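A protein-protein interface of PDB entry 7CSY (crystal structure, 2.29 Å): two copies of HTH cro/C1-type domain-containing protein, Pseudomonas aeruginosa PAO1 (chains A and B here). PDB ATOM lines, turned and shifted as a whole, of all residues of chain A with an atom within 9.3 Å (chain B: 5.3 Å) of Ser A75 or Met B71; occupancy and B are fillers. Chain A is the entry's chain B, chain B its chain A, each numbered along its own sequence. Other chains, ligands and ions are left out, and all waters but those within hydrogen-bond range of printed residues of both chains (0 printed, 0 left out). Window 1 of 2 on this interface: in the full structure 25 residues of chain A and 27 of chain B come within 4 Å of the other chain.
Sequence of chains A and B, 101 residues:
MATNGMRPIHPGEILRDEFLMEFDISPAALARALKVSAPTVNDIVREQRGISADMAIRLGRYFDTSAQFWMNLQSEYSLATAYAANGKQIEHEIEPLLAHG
The side-chain hydroxyl (OG) of Ser B75 lies within hydrogen-bond range of the side-chain amide nitrogen (NE2) of Gln A68 (3.1 Å).
OD1 of Asn B72 sits at hydrogen-bond distance from NE2 of Gln B68, at 3.2 Å. O of Asn B72 lies within hydrogen-bond range of OG of Ser B75 (3.3 Å). The side-chain amide oxygen (OD1) of Asn A72 sits at hydrogen-bond distance from the side-chain amide nitrogen (NE2) of Gln A68, 3.0 Å away. The backbone carbonyl oxygen (O) of Met A71 is in hydrogen-bond range of the side-chain hydroxyl (OG) of Ser A75 (3.4 Å). The side-chain hydroxyl (OG) of Ser A75 is in hydrogen-bond range of the backbone carbonyl oxygen (O) of Asn A72. The side-chain hydroxyl (OG) of Ser A78 lies within hydrogen-bond range of the side-chain amide nitrogen (NE2) of Gln A74 (2.7 Å).
Glu B76 touches Gln A68. Ser B75 touches Met A71. OD1 of Asn A72 touches OD1 of Asn B72, 3.9 Å away. NE2 of Gln B68 touches OG of Ser A75, 3.7 Å away. CE of Met B71 touches O of Ser A75, 3.5 Å away. OE1 of Gln B68 touches CA of Glu A76, at 3.3 Å. Ala B53 touches Ser A78. CD2 of Leu A79 touches CB of Ala B67, at 3.7 Å. Gln B68 touches Leu A79 (OE1 to CD2, 3.2 Å). Ala A82 touches Ala B53.
Ser A75 touches just these residues of chain B: Gln B68 (3.7 Å) and Met B71 (3.5 Å). Of chain A, only Ser A78 and Ala A82 come within 4 Å of Ala B53. Printed residues of chain B within 4 Å of Gln A68: Ser B75 (3.1 Å) and Glu B76 (3.5 Å). Of the printed residues of chain A, Ser B75 touches Gln A68 and Met A71. Printed residues of chain B within 4 Å of Asn A72: Asn B72. Printed residues of chain B within 4 Å of Ala A82: Ala B53 (3.5 Å). Printed residues of chain B within 4 Å of Ser A78: Ala B53. Trp A70 touches none of the printed residues of chain B. Ala A67 touches none of the printed residues of chain B. The nearest printed residue of chain B that does not touch Ser A78 is Met B71 (4.2 Å).
Of the 13 printed residues of chain B, 7 touch a printed residue of chain A. Printed residues of chain B that touch a printed residue of chain A: Ala B53, Ala B67, Gln B68, Met B71, Asn B72, Ser B75 and Glu B76. Hydrophobic or aromatic side chains of chain B within 4 Å of the printed part of chain A: Ala B53, Ala B67 and Met B71. Printed residues of chain A that touch a printed residue of chain B: Gln A68, Met A71, Asn A72, Ser A75, Glu A76, Ser A78, Leu A79 and Ala A82. Hydrophobic or aromatic side chains of chain A within 4 Å of the printed part of chain B: Met A71, Leu A79 and Ala A82. Among the printed residues, 11 pairs touch across the chains.
Gln A68 touches Ser B75, and with the chains exchanged Ser A75 touches Gln B68. Gln A68 touches Glu B76, and with the chains exchanged Glu A76 touches Gln B68. Met A71 touches Ser B75, and with the chains exchanged Ser A75 touches Met B71. Asn A72 touches its own counterpart, Asn B72. Positions printed for both chains: 52, 56, 67, 68, 69, 70, 71, 72, 73, 74, 75 and 76.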
ATOM      1  N   PRO A   8     -21.789 -17.299 -17.525  1.00  0.00           N
ATOM      2  CA  PRO A   8     -22.205 -17.006 -16.156  1.00  0.00           C
ATOM      3  C   PRO A   8     -23.558 -17.619 -15.834  1.00  0.00           C
ATOM      4  O   PRO A   8     -24.413 -17.827 -16.699  1.00  0.00           O
ATOM      5  CB  PRO A   8     -22.286 -15.479 -16.137  1.00  0.00           C
ATOM      6  CG  PRO A   8     -22.662 -15.120 -17.549  1.00  0.00           C
ATOM      7  CD  PRO A   8     -22.003 -16.150 -18.430  1.00  0.00           C
ATOM      8  N   ILE A   9     -23.748 -17.882 -14.565  1.00  0.00           N
ATOM      9  CA  ILE A   9     -24.987 -18.443 -14.075  1.00  0.00           C
ATOM     10  C   ILE A   9     -25.962 -17.313 -13.729  1.00  0.00           C
ATOM     11  O   ILE A   9     -25.601 -16.338 -13.059  1.00  0.00           O
ATOM     12  CB  ILE A   9     -24.701 -19.359 -12.877  1.00  0.00           C
ATOM     13  CG1 ILE A   9     -25.755 -20.434 -12.791  1.00  0.00           C
ATOM     14  CG2 ILE A   9     -24.422 -18.572 -11.572  1.00  0.00           C
ATOM     15  CD1 ILE A   9     -25.336 -21.590 -13.688  1.00  0.00           C
ATOM     16  N   HIS A  10     -27.192 -17.412 -14.235  1.00  0.00           N
ATOM     17  CA  HIS A  10     -28.192 -16.405 -13.922  1.00  0.00           C
ATOM     18  C   HIS A  10     -28.855 -16.742 -12.592  1.00  0.00           C
ATOM     19  O   HIS A  10     -29.120 -17.911 -12.322  1.00  0.00           O
ATOM     20  CB  HIS A  10     -29.241 -16.336 -15.022  1.00  0.00           C
ATOM     21  CG  HIS A  10     -30.188 -15.179 -14.908  1.00  0.00           C
ATOM     22  ND1 HIS A  10     -31.212 -15.133 -13.981  1.00  0.00           N
ATOM     23  CD2 HIS A  10     -30.287 -14.038 -15.629  1.00  0.00           C
ATOM     24  CE1 HIS A  10     -31.897 -14.018 -14.140  1.00  0.00           C
ATOM     25  NE2 HIS A  10     -31.360 -13.338 -15.137  1.00  0.00           N
ATOM     26  N   PRO A  11     -29.138 -15.736 -11.751  1.00  0.00           N
ATOM     27  CA  PRO A  11     -29.700 -16.032 -10.418  1.00  0.00           C
ATOM     28  C   PRO A  11     -31.016 -16.773 -10.470  1.00  0.00           C
ATOM     29  O   PRO A  11     -31.333 -17.522  -9.537  1.00  0.00           O
ATOM     30  CB  PRO A  11     -29.882 -14.643  -9.786  1.00  0.00           C
ATOM     31  CG  PRO A  11     -29.020 -13.742 -10.565  1.00  0.00           C
ATOM     32  CD  PRO A  11     -28.988 -14.292 -11.969  1.00  0.00           C
ATOM     33  N   GLY A  50     -33.224  -9.505 -13.974  1.00  0.00           N
ATOM     34  CA  GLY A  50     -32.304  -9.539 -12.867  1.00  0.00           C
ATOM     35  C   GLY A  50     -33.008  -9.457 -11.525  1.00  0.00           C
ATOM     36  O   GLY A  50     -34.179  -9.090 -11.429  1.00  0.00           O
ATOM     37  N   ILE A  51     -32.270  -9.814 -10.478  1.00  0.00           N
ATOM     38  CA  ILE A  51     -32.747  -9.653  -9.110  1.00  0.00           C
ATOM     39  C   ILE A  51     -32.437  -8.227  -8.653  1.00  0.00           C
ATOM     40  O   ILE A  51     -31.275  -7.870  -8.452  1.00  0.00           O
ATOM     41  CB  ILE A  51     -32.107 -10.684  -8.176  1.00  0.00           C
ATOM     42  CG1 ILE A  51     -32.434 -12.095  -8.684  1.00  0.00           C
ATOM     43  CG2 ILE A  51     -32.558 -10.468  -6.721  1.00  0.00           C
ATOM     44  CD1 ILE A  51     -32.338 -13.168  -7.634  1.00  0.00           C
ATOM     45  N   SER A  52     -33.478  -7.408  -8.505  1.00  0.00           N
ATOM     46  CA  SER A  52     -33.366  -6.103  -7.874  1.00  0.00           C
ATOM     47  C   SER A  52     -32.978  -6.235  -6.397  1.00  0.00           C
ATOM     48  O   SER A  52     -33.111  -7.295  -5.781  1.00  0.00           O
ATOM     49  CB  SER A  52     -34.695  -5.368  -7.977  1.00  0.00           C
ATOM     50  OG  SER A  52     -35.621  -5.971  -7.084  1.00  0.00           O
ATOM     51  N   ALA A  56     -34.042  -9.138  -3.779  1.00  0.00           N
ATOM     52  CA  ALA A  56     -33.114  -9.870  -2.927  1.00  0.00           C
ATOM     53  C   ALA A  56     -33.559  -9.854  -1.462  1.00  0.00           C
ATOM     54  O   ALA A  56     -33.330 -10.825  -0.728  1.00  0.00           O
ATOM     55  CB  ALA A  56     -31.715  -9.295  -3.082  1.00  0.00           C
ATOM     56  N   ALA A  67     -29.776 -12.023   2.154  1.00  0.00           N
ATOM     57  CA  ALA A  67     -30.123 -11.202   0.999  1.00  0.00           C
ATOM     58  C   ALA A  67     -28.905 -10.922   0.144  1.00  0.00           C
ATOM     59  O   ALA A  67     -29.018 -10.838  -1.083  1.00  0.00           O
ATOM     60  CB  ALA A  67     -30.776  -9.888   1.433  1.00  0.00           C
ATOM     61  N   GLN A  68     -27.732 -10.775   0.767  1.00  0.00           N
ATOM     62  CA  GLN A  68     -26.538 -10.458  -0.009  1.00  0.00           C
ATOM     63  C   GLN A  68     -26.140 -11.626  -0.911  1.00  0.00           C
ATOM     64  O   GLN A  68     -25.600 -11.406  -2.005  1.00  0.00           O
ATOM     65  CB  GLN A  68     -25.393 -10.045   0.925  1.00  0.00           C
ATOM     66  CG  GLN A  68     -24.130  -9.605   0.212  1.00  0.00           C
ATOM     67  CD  GLN A  68     -24.311  -8.285  -0.500  1.00  0.00           C
ATOM     68  OE1 GLN A  68     -24.830  -7.323   0.075  1.00  0.00           O
ATOM     69  NE2 GLN A  68     -23.879  -8.224  -1.756  1.00  0.00           N
ATOM     70  N   PHE A  69     -26.428 -12.867  -0.493  1.00  0.00           N
ATOM     71  CA  PHE A  69     -26.222 -14.017  -1.375  1.00  0.00           C
ATOM     72  C   PHE A  69     -26.855 -13.771  -2.741  1.00  0.00           C
ATOM     73  O   PHE A  69     -26.209 -13.928  -3.781  1.00  0.00           O
ATOM     74  CB  PHE A  69     -26.793 -15.269  -0.715  1.00  0.00           C
ATOM     75  CG  PHE A  69     -26.982 -16.437  -1.648  1.00  0.00           C
ATOM     76  CD1 PHE A  69     -25.922 -17.283  -1.944  1.00  0.00           C
ATOM     77  CD2 PHE A  69     -28.220 -16.703  -2.205  1.00  0.00           C
ATOM     78  CE1 PHE A  69     -26.082 -18.363  -2.774  1.00  0.00           C
ATOM     79  CE2 PHE A  69     -28.392 -17.792  -3.045  1.00  0.00           C
ATOM     80  CZ  PHE A  69     -27.321 -18.620  -3.330  1.00  0.00           C
ATOM     81  N   TRP A  70     -28.112 -13.324  -2.749  1.00  0.00           N
ATOM     82  CA  TRP A  70     -28.803 -13.037  -4.004  1.00  0.00           C
ATOM     83  C   TRP A  70     -28.168 -11.874  -4.751  1.00  0.00           C
ATOM     84  O   TRP A  70     -28.067 -11.924  -5.986  1.00  0.00           O
ATOM     85  CB  TRP A  70     -30.274 -12.755  -3.736  1.00  0.00           C
ATOM     86  CG  TRP A  70     -30.974 -13.955  -3.273  1.00  0.00           C
ATOM     87  CD1 TRP A  70     -31.425 -14.214  -2.023  1.00  0.00           C
ATOM     88  CD2 TRP A  70     -31.300 -15.094  -4.065  1.00  0.00           C
ATOM     89  NE1 TRP A  70     -32.025 -15.446  -1.984  1.00  0.00           N
ATOM     90  CE2 TRP A  70     -31.959 -16.007  -3.229  1.00  0.00           C
ATOM     91  CE3 TRP A  70     -31.107 -15.426  -5.406  1.00  0.00           C
ATOM     92  CZ2 TRP A  70     -32.423 -17.231  -3.684  1.00  0.00           C
ATOM     93  CZ3 TRP A  70     -31.569 -16.651  -5.854  1.00  0.00           C
ATOM     94  CH2 TRP A  70     -32.214 -17.533  -4.996  1.00  0.00           C
ATOM     95  N   MET A  71     -27.764 -10.803  -4.029  1.00  0.00           N
ATOM     96  CA  MET A  71     -27.082  -9.688  -4.688  1.00  0.00           C
ATOM     97  C   MET A  71     -25.775 -10.143  -5.312  1.00  0.00           C
ATOM     98  O   MET A  71     -25.377  -9.648  -6.377  1.00  0.00           O
ATOM     99  CB  MET A  71     -26.777  -8.539  -3.704  1.00  0.00           C
ATOM    100  CG  MET A  71     -27.967  -7.927  -2.996  1.00  0.00           C
ATOM    101  SD  MET A  71     -29.026  -6.961  -4.086  1.00  0.00           S
ATOM    102  CE  MET A  71     -28.023  -5.561  -4.530  1.00  0.00           C
ATOM    103  N   ASN A  72     -25.058 -11.033  -4.618  1.00  0.00           N
ATOM    104  CA  ASN A  72     -23.758 -11.475  -5.108  1.00  0.00           C
ATOM    105  C   ASN A  72     -23.907 -12.267  -6.391  1.00  0.00           C
ATOM    106  O   ASN A  72     -23.111 -12.103  -7.323  1.00  0.00           O
ATOM    107  CB  ASN A  72     -23.036 -12.309  -4.047  1.00  0.00           C
ATOM    108  CG  ASN A  72     -22.436 -11.455  -2.928  1.00  0.00           C
ATOM    109  OD1 ASN A  72     -22.181 -10.249  -3.095  1.00  0.00           O
ATOM    110  ND2 ASN A  72     -22.214 -12.081  -1.778  1.00  0.00           N
ATOM    111  N   LEU A  73     -24.935 -13.115  -6.466  1.00  0.00           N
ATOM    112  CA  LEU A  73     -25.213 -13.834  -7.708  1.00  0.00           C
ATOM    113  C   LEU A  73     -25.525 -12.856  -8.833  1.00  0.00           C
ATOM    114  O   LEU A  73     -24.989 -12.977  -9.940  1.00  0.00           O
ATOM    115  CB  LEU A  73     -26.376 -14.802  -7.506  1.00  0.00           C
ATOM    116  CG  LEU A  73     -26.114 -16.119  -6.790  1.00  0.00           C
ATOM    117  CD1 LEU A  73     -27.372 -16.961  -6.882  1.00  0.00           C
ATOM    118  CD2 LEU A  73     -24.928 -16.852  -7.421  1.00  0.00           C
ATOM    119  N   GLN A  74     -26.375 -11.858  -8.552  1.00  0.00           N
ATOM    120  CA  GLN A  74     -26.730 -10.889  -9.582  1.00  0.00           C
ATOM    121  C   GLN A  74     -25.520 -10.088 -10.048  1.00  0.00           C
ATOM    122  O   GLN A  74     -25.345  -9.869 -11.250  1.00  0.00           O
ATOM    123  CB  GLN A  74     -27.815  -9.934  -9.089  1.00  0.00           C
ATOM    124  CG  GLN A  74     -28.204  -8.917 -10.165  1.00  0.00           C
ATOM    125  CD  GLN A  74     -28.768  -9.623 -11.402  1.00  0.00           C
ATOM    126  OE1 GLN A  74     -29.635 -10.488 -11.288  1.00  0.00           O
ATOM    127  NE2 GLN A  74     -28.257  -9.272 -12.578  1.00  0.00           N
ATOM    128  N   SER A  75     -24.684  -9.608  -9.123  1.00  0.00           N
ATOM    129  CA  SER A  75     -23.621  -8.715  -9.571  1.00  0.00           C
ATOM    130  C   SER A  75     -22.572  -9.482 -10.362  1.00  0.00           C
ATOM    131  O   SER A  75     -22.124  -9.010 -11.410  1.00  0.00           O
ATOM    132  CB  SER A  75     -23.005  -7.947  -8.389  1.00  0.00           C
ATOM    133  OG  SER A  75     -22.260  -8.800  -7.553  1.00  0.00           O
ATOM    134  N   GLU A  76     -22.197 -10.677  -9.903  1.00  0.00           N
ATOM    135  CA  GLU A  76     -21.315 -11.534 -10.697  1.00  0.00           C
ATOM    136  C   GLU A  76     -21.904 -11.815 -12.079  1.00  0.00           C
ATOM    137  O   GLU A  76     -21.204 -11.714 -13.099  1.00  0.00           O
ATOM    138  CB  GLU A  76     -21.043 -12.843  -9.955  1.00  0.00           C
ATOM    139  CG  GLU A  76     -20.318 -12.650  -8.616  1.00  0.00           C
ATOM    140  CD  GLU A  76     -20.396 -13.889  -7.717  1.00  0.00           C
ATOM    141  OE1 GLU A  76     -21.045 -14.897  -8.105  1.00  0.00           O
ATOM    142  OE2 GLU A  76     -19.820 -13.839  -6.604  1.00  0.00           O
ATOM    143  N   TYR A  77     -23.200 -12.124 -12.141  1.00  0.00           N
ATOM    144  CA  TYR A  77     -23.818 -12.347 -13.445  1.00  0.00           C
ATOM    145  C   TYR A  77     -23.798 -11.082 -14.297  1.00  0.00           C
ATOM    146  O   TYR A  77     -23.474 -11.144 -15.490  1.00  0.00           O
ATOM    147  CB  TYR A  77     -25.243 -12.868 -13.294  1.00  0.00           C
ATOM    148  CG  TYR A  77     -25.888 -13.069 -14.640  1.00  0.00           C
ATOM    149  CD1 TYR A  77     -25.666 -14.229 -15.374  1.00  0.00           C
ATOM    150  CD2 TYR A  77     -26.689 -12.092 -15.190  1.00  0.00           C
ATOM    151  CE1 TYR A  77     -26.233 -14.394 -16.616  1.00  0.00           C
ATOM    152  CE2 TYR A  77     -27.265 -12.251 -16.418  1.00  0.00           C
ATOM    153  CZ  TYR A  77     -27.032 -13.401 -17.132  1.00  0.00           C
ATOM    154  OH  TYR A  77     -27.621 -13.538 -18.359  1.00  0.00           O
ATOM    155  N   SER A  78     -24.135  -9.921 -13.703  1.00  0.00           N
ATOM    156  CA  SER A  78     -24.124  -8.661 -14.448  1.00  0.00           C
ATOM    157  C   SER A  78     -22.721  -8.259 -14.848  1.00  0.00           C
ATOM    158  O   SER A  78     -22.533  -7.632 -15.897  1.00  0.00           O
ATOM    159  CB  SER A  78     -24.741  -7.525 -13.632  1.00  0.00           C
ATOM    160  OG  SER A  78     -26.093  -7.791 -13.326  1.00  0.00           O
ATOM    161  N   LEU A  79     -21.736  -8.560 -14.003  1.00  0.00           N
ATOM    162  CA  LEU A  79     -20.358  -8.248 -14.358  1.00  0.00           C
ATOM    163  C   LEU A  79     -19.897  -9.121 -15.516  1.00  0.00           C
ATOM    164  O   LEU A  79     -19.341  -8.619 -16.501  1.00  0.00           O
ATOM    165  CB  LEU A  79     -19.434  -8.422 -13.151  1.00  0.00           C
ATOM    166  CG  LEU A  79     -17.977  -8.184 -13.554  1.00  0.00           C
ATOM    167  CD1 LEU A  79     -17.802  -6.780 -14.137  1.00  0.00           C
ATOM    168  CD2 LEU A  79     -17.000  -8.423 -12.397  1.00  0.00           C
ATOM    169  N   ALA A  80     -20.148 -10.432 -15.413  1.00  0.00           N
ATOM    170  CA  ALA A  80     -19.712 -11.371 -16.444  1.00  0.00           C
ATOM    171  C   ALA A  80     -20.354 -11.062 -17.789  1.00  0.00           C
ATOM    172  O   ALA A  80     -19.684 -11.081 -18.826  1.00  0.00           O
ATOM    173  CB  ALA A  80     -20.027 -12.800 -16.010  1.00  0.00           C
ATOM    174  N   THR A  81     -21.642 -10.732 -17.787  1.00  0.00           N
ATOM    175  CA  THR A  81     -22.319 -10.435 -19.041  1.00  0.00           C
ATOM    176  C   THR A  81     -21.920  -9.058 -19.586  1.00  0.00           C
ATOM    177  O   THR A  81     -21.801  -8.881 -20.799  1.00  0.00           O
ATOM    178  CB  THR A  81     -23.832 -10.578 -18.836  1.00  0.00           C
ATOM    179  OG1 THR A  81     -24.504 -10.401 -20.080  1.00  0.00           O
ATOM    180  CG2 THR A  81     -24.339  -9.536 -17.911  1.00  0.00           C
ATOM    181  N   ALA A  82     -21.657  -8.084 -18.714  1.00  0.00           N
ATOM    182  CA  ALA A  82     -21.102  -6.815 -19.175  1.00  0.00           C
ATOM    183  C   ALA A  82     -19.709  -7.004 -19.758  1.00  0.00           C
ATOM    184  O   ALA A  82     -19.352  -6.366 -20.753  1.00  0.00           O
ATOM    185  CB  ALA A  82     -21.044  -5.816 -18.026  1.00  0.00           C
ATOM    186  N   TYR A  83     -18.901  -7.865 -19.144  1.00  0.00           N
ATOM    187  CA  TYR A  83     -17.534  -8.033 -19.612  1.00  0.00           C
ATOM    188  C   TYR A  83     -17.471  -8.774 -20.945  1.00  0.00           C
ATOM    189  O   TYR A  83     -16.636  -8.447 -21.792  1.00  0.00           O
ATOM    190  CB  TYR A  83     -16.705  -8.766 -18.573  1.00  0.00           C
ATOM    191  CG  TYR A  83     -15.244  -8.677 -18.899  1.00  0.00           C
ATOM    192  CD1 TYR A  83     -14.509  -7.555 -18.550  1.00  0.00           C
ATOM    193  CD2 TYR A  83     -14.603  -9.691 -19.590  1.00  0.00           C
ATOM    194  CE1 TYR A  83     -13.171  -7.452 -18.856  1.00  0.00           C
ATOM    195  CE2 TYR A  83     -13.262  -9.601 -19.898  1.00  0.00           C
ATOM    196  CZ  TYR A  83     -12.559  -8.477 -19.528  1.00  0.00           C
ATOM    197  OH  TYR A  83     -11.229  -8.385 -19.833  1.00  0.00           O
ATOM    198  N   SER B  52     -22.258   1.350 -12.446  1.00  0.00           N
ATOM    199  CA  SER B  52     -22.751   0.355 -13.386  1.00  0.00           C
ATOM    200  C   SER B  52     -21.688  -0.731 -13.579  1.00  0.00           C
ATOM    201  O   SER B  52     -20.513  -0.551 -13.230  1.00  0.00           O
ATOM    202  CB  SER B  52     -23.090   1.005 -14.728  1.00  0.00           C
ATOM    203  OG  SER B  52     -21.909   1.498 -15.360  1.00  0.00           O
ATOM    204  N   ALA B  53     -22.107  -1.873 -14.141  1.00  0.00           N
ATOM    205  CA  ALA B  53     -21.147  -2.938 -14.437  1.00  0.00           C
ATOM    206  C   ALA B  53     -20.063  -2.448 -15.393  1.00  0.00           C
ATOM    207  O   ALA B  53     -18.881  -2.775 -15.241  1.00  0.00           O
ATOM    208  CB  ALA B  53     -21.871  -4.157 -15.028  1.00  0.00           C
ATOM    209  N   ALA B  56     -17.725  -0.391 -13.422  1.00  0.00           N
ATOM    210  CA  ALA B  56     -16.881  -1.251 -12.591  1.00  0.00           C
ATOM    211  C   ALA B  56     -15.755  -1.871 -13.389  1.00  0.00           C
ATOM    212  O   ALA B  56     -14.691  -2.151 -12.843  1.00  0.00           O
ATOM    213  CB  ALA B  56     -17.688  -2.383 -11.938  1.00  0.00           C
ATOM    214  N   ALA B  67     -12.858  -5.831 -10.944  1.00  0.00           N
ATOM    215  CA  ALA B  67     -14.148  -5.202 -11.189  1.00  0.00           C
ATOM    216  C   ALA B  67     -15.151  -5.621 -10.123  1.00  0.00           C
ATOM    217  O   ALA B  67     -15.937  -4.792  -9.648  1.00  0.00           O
ATOM    218  CB  ALA B  67     -14.654  -5.543 -12.586  1.00  0.00           C
ATOM    219  N   GLN B  68     -15.101  -6.888  -9.698  1.00  0.00           N
ATOM    220  CA  GLN B  68     -16.018  -7.351  -8.659  1.00  0.00           C
ATOM    221  C   GLN B  68     -15.927  -6.475  -7.421  1.00  0.00           C
ATOM    222  O   GLN B  68     -16.925  -6.312  -6.709  1.00  0.00           O
ATOM    223  CB  GLN B  68     -15.737  -8.805  -8.252  1.00  0.00           C
ATOM    224  CG  GLN B  68     -16.585  -9.844  -8.913  1.00  0.00           C
ATOM    225  CD  GLN B  68     -18.061  -9.545  -8.898  1.00  0.00           C
ATOM    226  OE1 GLN B  68     -18.706  -9.623  -9.933  1.00  0.00           O
ATOM    227  NE2 GLN B  68     -18.613  -9.227  -7.734  1.00  0.00           N
ATOM    228  N   PHE B  69     -14.740  -5.931  -7.133  1.00  0.00           N
ATOM    229  CA  PHE B  69     -14.592  -5.041  -5.982  1.00  0.00           C
ATOM    230  C   PHE B  69     -15.594  -3.892  -6.066  1.00  0.00           C
ATOM    231  O   PHE B  69     -16.356  -3.637  -5.126  1.00  0.00           O
ATOM    232  CB  PHE B  69     -13.146  -4.529  -5.905  1.00  0.00           C
ATOM    233  CG  PHE B  69     -12.943  -3.328  -4.987  1.00  0.00           C
ATOM    234  CD1 PHE B  69     -12.831  -3.489  -3.615  1.00  0.00           C
ATOM    235  CD2 PHE B  69     -12.837  -2.045  -5.511  1.00  0.00           C
ATOM    236  CE1 PHE B  69     -12.628  -2.397  -2.785  1.00  0.00           C
ATOM    237  CE2 PHE B  69     -12.632  -0.930  -4.667  1.00  0.00           C
ATOM    238  CZ  PHE B  69     -12.531  -1.107  -3.316  1.00  0.00           C
ATOM    239  N   TRP B  70     -15.661  -3.246  -7.223  1.00  0.00           N
ATOM    240  CA  TRP B  70     -16.609  -2.155  -7.403  1.00  0.00           C
ATOM    241  C   TRP B  70     -18.052  -2.644  -7.383  1.00  0.00           C
ATOM    242  O   TRP B  70     -18.925  -1.962  -6.827  1.00  0.00           O
ATOM    243  CB  TRP B  70     -16.282  -1.430  -8.697  1.00  0.00           C
ATOM    244  CG  TRP B  70     -14.944  -0.802  -8.582  1.00  0.00           C
ATOM    245  CD1 TRP B  70     -13.762  -1.254  -9.099  1.00  0.00           C
ATOM    246  CD2 TRP B  70     -14.639   0.399  -7.863  1.00  0.00           C
ATOM    247  NE1 TRP B  70     -12.739  -0.397  -8.746  1.00  0.00           N
ATOM    248  CE2 TRP B  70     -13.258   0.627  -7.993  1.00  0.00           C
ATOM    249  CE3 TRP B  70     -15.406   1.307  -7.133  1.00  0.00           C
ATOM    250  CZ2 TRP B  70     -12.629   1.725  -7.408  1.00  0.00           C
ATOM    251  CZ3 TRP B  70     -14.769   2.399  -6.550  1.00  0.00           C
ATOM    252  CH2 TRP B  70     -13.403   2.594  -6.698  1.00  0.00           C
ATOM    253  N   MET B  71     -18.328  -3.816  -7.986  1.00  0.00           N
ATOM    254  CA  MET B  71     -19.687  -4.354  -7.946  1.00  0.00           C
ATOM    255  C   MET B  71     -20.103  -4.661  -6.516  1.00  0.00           C
ATOM    256  O   MET B  71     -21.259  -4.424  -6.134  1.00  0.00           O
ATOM    257  CB  MET B  71     -19.820  -5.618  -8.809  1.00  0.00           C
ATOM    258  CG  MET B  71     -19.297  -5.511 -10.241  1.00  0.00           C
ATOM    259  SD  MET B  71     -20.378  -4.601 -11.358  1.00  0.00           S
ATOM    260  CE  MET B  71     -21.905  -5.556 -11.313  1.00  0.00           C
ATOM    261  N   ASN B  72     -19.176  -5.190  -5.709  1.00  0.00           N
ATOM    262  CA  ASN B  72     -19.505  -5.512  -4.323  1.00  0.00           C
ATOM    263  C   ASN B  72     -19.771  -4.252  -3.512  1.00  0.00           C
ATOM    264  O   ASN B  72     -20.658  -4.246  -2.651  1.00  0.00           O
ATOM    265  CB  ASN B  72     -18.392  -6.339  -3.681  1.00  0.00           C
ATOM    266  CG  ASN B  72     -18.313  -7.753  -4.250  1.00  0.00           C
ATOM    267  OD1 ASN B  72     -19.285  -8.283  -4.797  1.00  0.00           O
ATOM    268  ND2 ASN B  72     -17.153  -8.366  -4.121  1.00  0.00           N
ATOM    269  N   LEU B  73     -19.021  -3.174  -3.763  1.00  0.00           N
ATOM    270  CA  LEU B  73     -19.332  -1.921  -3.082  1.00  0.00           C
ATOM    271  C   LEU B  73     -20.711  -1.438  -3.486  1.00  0.00           C
ATOM    272  O   LEU B  73     -21.508  -1.024  -2.638  1.00  0.00           O
ATOM    273  CB  LEU B  73     -18.292  -0.843  -3.402  1.00  0.00           C
ATOM    274  CG  LEU B  73     -16.883  -0.911  -2.826  1.00  0.00           C
ATOM    275  CD1 LEU B  73     -15.974   0.007  -3.606  1.00  0.00           C
ATOM    276  CD2 LEU B  73     -16.869  -0.544  -1.345  1.00  0.00           C
ATOM    277  N   GLN B  74     -21.025  -1.526  -4.781  1.00  0.00           N
ATOM    278  CA  GLN B  74     -22.325  -1.074  -5.241  1.00  0.00           C
ATOM    279  C   GLN B  74     -23.440  -1.956  -4.697  1.00  0.00           C
ATOM    280  O   GLN B  74     -24.476  -1.449  -4.250  1.00  0.00           O
ATOM    281  CB  GLN B  74     -22.360  -1.025  -6.765  1.00  0.00           C
ATOM    282  CG  GLN B  74     -23.660  -0.454  -7.280  1.00  0.00           C
ATOM    283  CD  GLN B  74     -23.927   0.959  -6.729  1.00  0.00           C
ATOM    284  OE1 GLN B  74     -23.116   1.871  -6.905  1.00  0.00           O
ATOM    285  NE2 GLN B  74     -25.064   1.132  -6.058  1.00  0.00           N
ATOM    286  N   SER B  75     -23.235  -3.275  -4.680  1.00  0.00           N
ATOM    287  CA  SER B  75     -24.341  -4.149  -4.326  1.00  0.00           C
ATOM    288  C   SER B  75     -24.637  -4.069  -2.840  1.00  0.00           C
ATOM    289  O   SER B  75     -25.804  -4.108  -2.427  1.00  0.00           O
ATOM    290  CB  SER B  75     -24.041  -5.579  -4.749  1.00  0.00           C
ATOM    291  OG  SER B  75     -23.092  -6.169  -3.888  1.00  0.00           O
ATOM    292  N   GLU B  76     -23.595  -3.947  -2.023  1.00  0.00           N
ATOM    293  CA  GLU B  76     -23.811  -3.758  -0.593  1.00  0.00           C
ATOM    294  C   GLU B  76     -24.483  -2.417  -0.320  1.00  0.00           C
ATOM    295  O   GLU B  76     -25.392  -2.329   0.516  1.00  0.00           O
ATOM    296  CB  GLU B  76     -22.486  -3.883   0.154  1.00  0.00           C
ATOM    297  CG  GLU B  76     -21.922  -5.325   0.135  1.00  0.00           C
ATOM    298  CD  GLU B  76     -20.406  -5.397   0.387  1.00  0.00           C
ATOM    299  OE1 GLU B  76     -19.815  -6.490   0.156  1.00  0.00           O
ATOM    300  OE2 GLU B  76     -19.809  -4.362   0.808  1.00  0.00           O
